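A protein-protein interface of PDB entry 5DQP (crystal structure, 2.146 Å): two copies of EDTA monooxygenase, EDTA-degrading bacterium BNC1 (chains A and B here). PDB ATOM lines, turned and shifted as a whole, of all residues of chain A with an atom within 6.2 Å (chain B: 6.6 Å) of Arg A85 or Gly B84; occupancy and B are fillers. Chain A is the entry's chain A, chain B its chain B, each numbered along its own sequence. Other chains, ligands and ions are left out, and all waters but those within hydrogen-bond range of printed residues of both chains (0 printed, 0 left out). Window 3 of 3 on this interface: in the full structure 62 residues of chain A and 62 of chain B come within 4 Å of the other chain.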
ATOM      1  N   LEU A  35      27.864   9.134 -25.485  1.00  0.00           N
ATOM      2  CA  LEU A  35      27.834   9.602 -24.106  1.00  0.00           C
ATOM      3  C   LEU A  35      29.194  10.152 -23.671  1.00  0.00           C
ATOM      4  O   LEU A  35      29.269  11.161 -22.953  1.00  0.00           O
ATOM      5  CB  LEU A  35      27.387   8.465 -23.180  1.00  0.00           C
ATOM      6  CG  LEU A  35      27.421   8.756 -21.677  1.00  0.00           C
ATOM      7  CD1 LEU A  35      26.489   9.967 -21.323  1.00  0.00           C
ATOM      8  CD2 LEU A  35      27.063   7.464 -20.897  1.00  0.00           C
ATOM      9  N   GLU A  36      30.282   9.506 -24.098  1.00  0.00           N
ATOM     10  CA  GLU A  36      31.609   9.945 -23.675  1.00  0.00           C
ATOM     11  C   GLU A  36      31.917  11.358 -24.147  1.00  0.00           C
ATOM     12  O   GLU A  36      32.672  12.078 -23.484  1.00  0.00           O
ATOM     13  CB  GLU A  36      32.673   8.969 -24.171  1.00  0.00           C
ATOM     14  CG  GLU A  36      32.555   7.568 -23.550  1.00  0.00           C
ATOM     15  CD  GLU A  36      32.543   7.581 -22.017  1.00  0.00           C
ATOM     16  OE1 GLU A  36      33.332   8.360 -21.419  1.00  0.00           O
ATOM     17  OE2 GLU A  36      31.746   6.815 -21.418  1.00  0.00           O
ATOM     18  N   ILE A  39      30.472  13.149 -21.243  1.00  0.00           N
ATOM     19  CA  ILE A  39      31.261  12.908 -20.039  1.00  0.00           C
ATOM     20  C   ILE A  39      32.518  13.761 -20.077  1.00  0.00           C
ATOM     21  O   ILE A  39      32.877  14.415 -19.090  1.00  0.00           O
ATOM     22  CB  ILE A  39      31.612  11.413 -19.889  1.00  0.00           C
ATOM     23  CG1 ILE A  39      30.357  10.536 -19.863  1.00  0.00           C
ATOM     24  CG2 ILE A  39      32.450  11.184 -18.617  1.00  0.00           C
ATOM     25  CD1 ILE A  39      29.374  10.905 -18.788  1.00  0.00           C
ATOM     26  N   GLU A  43      33.278  16.412 -17.187  1.00  0.00           N
ATOM     27  CA  GLU A  43      34.468  16.256 -16.345  1.00  0.00           C
ATOM     28  C   GLU A  43      35.411  17.457 -16.472  1.00  0.00           C
ATOM     29  O   GLU A  43      36.099  17.811 -15.507  1.00  0.00           O
ATOM     30  CB  GLU A  43      35.203  14.957 -16.696  1.00  0.00           C
ATOM     31  CG  GLU A  43      34.587  13.644 -16.141  1.00  0.00           C
ATOM     32  CD  GLU A  43      34.810  13.391 -14.616  1.00  0.00           C
ATOM     33  OE1 GLU A  43      34.438  12.285 -14.145  1.00  0.00           O
ATOM     34  OE2 GLU A  43      35.343  14.272 -13.885  1.00  0.00           O
ATOM     35  N   ALA A  80      20.692  12.419 -16.661  1.00  0.00           N
ATOM     36  CA  ALA A  80      20.746  11.245 -15.787  1.00  0.00           C
ATOM     37  C   ALA A  80      21.993  10.404 -16.046  1.00  0.00           C
ATOM     38  O   ALA A  80      22.612   9.900 -15.104  1.00  0.00           O
ATOM     39  CB  ALA A  80      19.487  10.391 -15.971  1.00  0.00           C
ATOM     40  N   ALA A  81      22.356  10.206 -17.317  1.00  0.00           N
ATOM     41  CA  ALA A  81      23.525   9.378 -17.630  1.00  0.00           C
ATOM     42  C   ALA A  81      24.811  10.090 -17.246  1.00  0.00           C
ATOM     43  O   ALA A  81      25.700   9.497 -16.623  1.00  0.00           O
ATOM     44  CB  ALA A  81      23.547   9.019 -19.118  1.00  0.00           C
ATOM     45  N   ILE A  82      24.914  11.374 -17.579  1.00  0.00           N
ATOM     46  CA  ILE A  82      26.077  12.161 -17.169  1.00  0.00           C
ATOM     47  C   ILE A  82      26.286  12.087 -15.659  1.00  0.00           C
ATOM     48  O   ILE A  82      27.378  11.757 -15.182  1.00  0.00           O
ATOM     49  CB  ILE A  82      25.931  13.629 -17.609  1.00  0.00           C
ATOM     50  CG1 ILE A  82      25.900  13.746 -19.141  1.00  0.00           C
ATOM     51  CG2 ILE A  82      27.095  14.445 -17.006  1.00  0.00           C
ATOM     52  CD1 ILE A  82      25.723  15.246 -19.657  1.00  0.00           C
ATOM     53  N   THR A  83      25.275  12.489 -14.882  1.00  0.00           N
ATOM     54  CA  THR A  83      25.495  12.578 -13.440  1.00  0.00           C
ATOM     55  C   THR A  83      25.549  11.212 -12.775  1.00  0.00           C
ATOM     56  O   THR A  83      26.113  11.101 -11.679  1.00  0.00           O
ATOM     57  CB  THR A  83      24.444  13.461 -12.757  1.00  0.00           C
ATOM     58  OG1 THR A  83      23.136  12.905 -12.933  1.00  0.00           O
ATOM     59  CG2 THR A  83      24.506  14.903 -13.344  1.00  0.00           C
ATOM     60  N   GLY A  84      25.028  10.167 -13.421  1.00  0.00           N
ATOM     61  CA  GLY A  84      25.319   8.824 -12.949  1.00  0.00           C
ATOM     62  C   GLY A  84      26.805   8.538 -12.907  1.00  0.00           C
ATOM     63  O   GLY A  84      27.258   7.723 -12.104  1.00  0.00           O
ATOM     64  N   ARG A  85      27.583   9.224 -13.748  1.00  0.00           N
ATOM     65  CA  ARG A  85      29.000   8.970 -13.964  1.00  0.00           C
ATOM     66  C   ARG A  85      29.911  10.056 -13.404  1.00  0.00           C
ATOM     67  O   ARG A  85      30.982   9.749 -12.878  1.00  0.00           O
ATOM     68  CB  ARG A  85      29.278   8.819 -15.469  1.00  0.00           C
ATOM     69  CG  ARG A  85      30.771   8.894 -15.824  1.00  0.00           C
ATOM     70  CD  ARG A  85      31.385   7.512 -15.992  1.00  0.00           C
ATOM     71  NE  ARG A  85      30.611   6.745 -16.967  1.00  0.00           N
ATOM     72  CZ  ARG A  85      30.968   6.530 -18.228  1.00  0.00           C
ATOM     73  NH1 ARG A  85      30.173   5.824 -19.021  1.00  0.00           N
ATOM     74  NH2 ARG A  85      32.120   7.007 -18.695  1.00  0.00           N
ATOM     75  N   VAL A  86      29.528  11.318 -13.502  1.00  0.00           N
ATOM     76  CA  VAL A  86      30.354  12.446 -13.081  1.00  0.00           C
ATOM     77  C   VAL A  86      29.776  12.999 -11.779  1.00  0.00           C
ATOM     78  O   VAL A  86      28.633  13.463 -11.772  1.00  0.00           O
ATOM     79  CB  VAL A  86      30.401  13.524 -14.170  1.00  0.00           C
ATOM     80  CG1 VAL A  86      31.364  14.638 -13.790  1.00  0.00           C
ATOM     81  CG2 VAL A  86      30.778  12.885 -15.534  1.00  0.00           C
ATOM     82  N   PRO A  87      30.521  12.984 -10.676  1.00  0.00           N
ATOM     83  CA  PRO A  87      30.024  13.556  -9.418  1.00  0.00           C
ATOM     84  C   PRO A  87      30.117  15.082  -9.389  1.00  0.00           C
ATOM     85  O   PRO A  87      30.656  15.717 -10.293  1.00  0.00           O
ATOM     86  CB  PRO A  87      30.946  12.936  -8.371  1.00  0.00           C
ATOM     87  CG  PRO A  87      32.239  12.727  -9.103  1.00  0.00           C
ATOM     88  CD  PRO A  87      31.854  12.371 -10.526  1.00  0.00           C
ATOM     89  N   LEU B  35      20.771   5.921  -5.686  1.00  0.00           N
ATOM     90  CA  LEU B  35      21.299   5.324  -6.914  1.00  0.00           C
ATOM     91  C   LEU B  35      22.184   4.104  -6.632  1.00  0.00           C
ATOM     92  O   LEU B  35      22.112   3.103  -7.353  1.00  0.00           O
ATOM     93  CB  LEU B  35      22.081   6.370  -7.716  1.00  0.00           C
ATOM     94  CG  LEU B  35      22.757   5.834  -8.985  1.00  0.00           C
ATOM     95  CD1 LEU B  35      21.712   5.215  -9.922  1.00  0.00           C
ATOM     96  CD2 LEU B  35      23.540   6.940  -9.724  1.00  0.00           C
ATOM     97  N   ALA B  79      17.160   3.957 -15.407  1.00  0.00           N
ATOM     98  CA  ALA B  79      17.950   3.167 -16.354  1.00  0.00           C
ATOM     99  C   ALA B  79      19.078   3.988 -16.974  1.00  0.00           C
ATOM    100  O   ALA B  79      20.166   3.465 -17.251  1.00  0.00           O
ATOM    101  CB  ALA B  79      17.058   2.606 -17.463  1.00  0.00           C
ATOM    102  N   ALA B  80      18.818   5.260 -17.264  1.00  0.00           N
ATOM    103  CA  ALA B  80      19.873   6.094 -17.812  1.00  0.00           C
ATOM    104  C   ALA B  80      21.027   6.217 -16.814  1.00  0.00           C
ATOM    105  O   ALA B  80      22.199   6.089 -17.184  1.00  0.00           O
ATOM    106  CB  ALA B  80      19.301   7.460 -18.177  1.00  0.00           C
ATOM    107  N   ALA B  81      20.702   6.441 -15.539  1.00  0.00           N
ATOM    108  CA  ALA B  81      21.730   6.577 -14.513  1.00  0.00           C
ATOM    109  C   ALA B  81      22.514   5.284 -14.334  1.00  0.00           C
ATOM    110  O   ALA B  81      23.747   5.308 -14.261  1.00  0.00           O
ATOM    111  CB  ALA B  81      21.095   7.003 -13.196  1.00  0.00           C
ATOM    112  N   ILE B  82      21.813   4.142 -14.242  1.00  0.00           N
ATOM    113  CA  ILE B  82      22.484   2.854 -14.034  1.00  0.00           C
ATOM    114  C   ILE B  82      23.427   2.537 -15.190  1.00  0.00           C
ATOM    115  O   ILE B  82      24.598   2.195 -14.982  1.00  0.00           O
ATOM    116  CB  ILE B  82      21.461   1.725 -13.861  1.00  0.00           C
ATOM    117  CG1 ILE B  82      20.670   1.874 -12.558  1.00  0.00           C
ATOM    118  CG2 ILE B  82      22.176   0.362 -13.930  1.00  0.00           C
ATOM    119  CD1 ILE B  82      19.488   0.941 -12.533  1.00  0.00           C
ATOM    120  N   THR B  83      22.924   2.619 -16.429  1.00  0.00           N
ATOM    121  CA  THR B  83      23.761   2.250 -17.559  1.00  0.00           C
ATOM    122  C   THR B  83      24.867   3.267 -17.806  1.00  0.00           C
ATOM    123  O   THR B  83      25.871   2.919 -18.425  1.00  0.00           O
ATOM    124  CB  THR B  83      22.941   2.043 -18.846  1.00  0.00           C
ATOM    125  OG1 THR B  83      22.120   3.180 -19.137  1.00  0.00           O
ATOM    126  CG2 THR B  83      22.085   0.776 -18.758  1.00  0.00           C
ATOM    127  N   GLY B  84      24.708   4.508 -17.342  1.00  0.00           N
ATOM    128  CA  GLY B  84      25.825   5.439 -17.387  1.00  0.00           C
ATOM    129  C   GLY B  84      26.998   4.978 -16.543  1.00  0.00           C
ATOM    130  O   GLY B  84      28.154   5.240 -16.879  1.00  0.00           O
ATOM    131  N   ARG B  85      26.724   4.257 -15.457  1.00  0.00           N
ATOM    132  CA  ARG B  85      27.757   3.807 -14.533  1.00  0.00           C
ATOM    133  C   ARG B  85      28.183   2.353 -14.759  1.00  0.00           C
ATOM    134  O   ARG B  85      29.375   2.037 -14.632  1.00  0.00           O
ATOM    135  CB  ARG B  85      27.261   3.977 -13.090  1.00  0.00           C
ATOM    136  CG  ARG B  85      28.180   3.328 -12.058  1.00  0.00           C
ATOM    137  CD  ARG B  85      29.115   4.364 -11.422  1.00  0.00           C
ATOM    138  NE  ARG B  85      28.343   5.488 -10.892  1.00  0.00           N
ATOM    139  CZ  ARG B  85      27.910   5.580  -9.638  1.00  0.00           C
ATOM    140  NH1 ARG B  85      28.187   4.622  -8.761  1.00  0.00           N
ATOM    141  NH2 ARG B  85      27.201   6.630  -9.262  1.00  0.00           N
ATOM    142  N   VAL B  86      27.251   1.470 -15.100  1.00  0.00           N
ATOM    143  CA  VAL B  86      27.476   0.029 -15.184  1.00  0.00           C
ATOM    144  C   VAL B  86      27.504  -0.381 -16.656  1.00  0.00           C
ATOM    145  O   VAL B  86      26.506  -0.195 -17.367  1.00  0.00           O
ATOM    146  CB  VAL B  86      26.401  -0.753 -14.410  1.00  0.00           C
ATOM    147  CG1 VAL B  86      26.678  -2.258 -14.469  1.00  0.00           C
ATOM    148  CG2 VAL B  86      26.308  -0.220 -12.930  1.00  0.00           C
ATOM    149  N   PRO B  87      28.596  -0.974 -17.138  1.00  0.00           N
ATOM    150  CA  PRO B  87      28.681  -1.423 -18.538  1.00  0.00           C
ATOM    151  C   PRO B  87      27.981  -2.760 -18.782  1.00  0.00           C
ATOM    152  O   PRO B  87      27.518  -3.434 -17.858  1.00  0.00           O
ATOM    153  CB  PRO B  87      30.193  -1.561 -18.756  1.00  0.00           C
ATOM    154  CG  PRO B  87      30.694  -2.021 -17.368  1.00  0.00           C
ATOM    155  CD  PRO B  87      29.857  -1.198 -16.394  1.00  0.00           C
ATOM    156  N   SER B 116      23.417   4.452 -24.121  1.00  0.00           N
ATOM    157  CA  SER B 116      24.008   3.303 -23.441  1.00  0.00           C
ATOM    158  C   SER B 116      24.760   2.381 -24.392  1.00  0.00           C
ATOM    159  O   SER B 116      25.166   1.291 -23.986  1.00  0.00           O
ATOM    160  CB  SER B 116      22.936   2.481 -22.703  1.00  0.00           C
ATOM    161  OG  SER B 116      21.993   1.956 -23.636  1.00  0.00           O
ATOM    162  N   ARG B 119      21.788  -0.636 -25.254  1.00  0.00           N
ATOM    163  CA  ARG B 119      21.496  -1.605 -24.210  1.00  0.00           C
ATOM    164  C   ARG B 119      20.070  -1.516 -23.621  1.00  0.00           C
ATOM    165  O   ARG B 119      19.792  -2.174 -22.616  1.00  0.00           O
ATOM    166  CB  ARG B 119      22.551  -1.449 -23.112  1.00  0.00           C
ATOM    167  CG  ARG B 119      23.917  -2.054 -23.504  1.00  0.00           C
ATOM    168  CD  ARG B 119      24.818  -2.055 -22.282  1.00  0.00           C
ATOM    169  NE  ARG B 119      25.364  -0.724 -21.933  1.00  0.00           N
ATOM    170  CZ  ARG B 119      25.519  -0.283 -20.677  1.00  0.00           C
ATOM    171  NH1 ARG B 119      26.069   0.902 -20.449  1.00  0.00           N
ATOM    172  NH2 ARG B 119      25.123  -1.019 -19.639  1.00  0.00           N
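The guanidinium group (NH2) of Arg A85 is in salt-bridge range of the side-chain carboxylate (OE2) of Glu A36.
Ala A80 touches its own counterpart, Ala B80.
Ala A80 touches Ala B81, and with the chains exchanged Ala A81 touches Ala B80.
Gly A84 touches Arg B85, and with the chains exchanged Arg A85 touches Gly B84.
Positions printed for both chains: 35, 80, 81, 82, 83, 84, 85, 86 and 87.
Of the 5 pairs that touch across the chains among the printed residues, 5 have their exchanged pair printed and touching as well.
Of the printed residues of chain A, Gly B84 touches Arg A85.
Of the printed residues of chain A, Arg B85 touches Gly A84.
Of the printed residues of chain A, Ala B80 touches Ala A80 (3.7 Å) and Ala A81 (3.6 Å).
Printed residues of chain B within 4 Å of Gly A84: Arg B85.
Of the printed residues of chain A, Ala B81 touches Ala A80.
The nearest printed residue of chain A that does not touch Ala B81 is Gly A84 (4.1 Å).
Printed residues of chain A that touch a printed residue of chain B: Ala A80, Ala A81, Gly A84 and Arg A85.
Along chain A the printed residues that touch a printed residue of chain B span positions 80 to 85.
Hydrophobic or aromatic side chains of chain B within 4 Å of the printed part of chain A: Ala B80 and Ala B81.
Among the printed residues, 5 pairs touch across the chains.
Among the printed residues, no Asp or Glu carboxylate lies within 4 Å of a Lys or Arg side-chain nitrogen of the other chain.
Among the printed residues, pairs that only touch across the chains: Ala A80 with Ala B80, Ala A80 with Ala B81 and Ala A81 with Ala B80.
The guanidinium group of Arg B85 lies within hydrogen-bond range of the backbone carbonyl oxygen of Gly A84 (2.8 Å).
The backbone carbonyl oxygen (O) of Gly B84 is in hydrogen-bond range of the guanidinium group (NE) of Arg A85 (2.9 Å).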
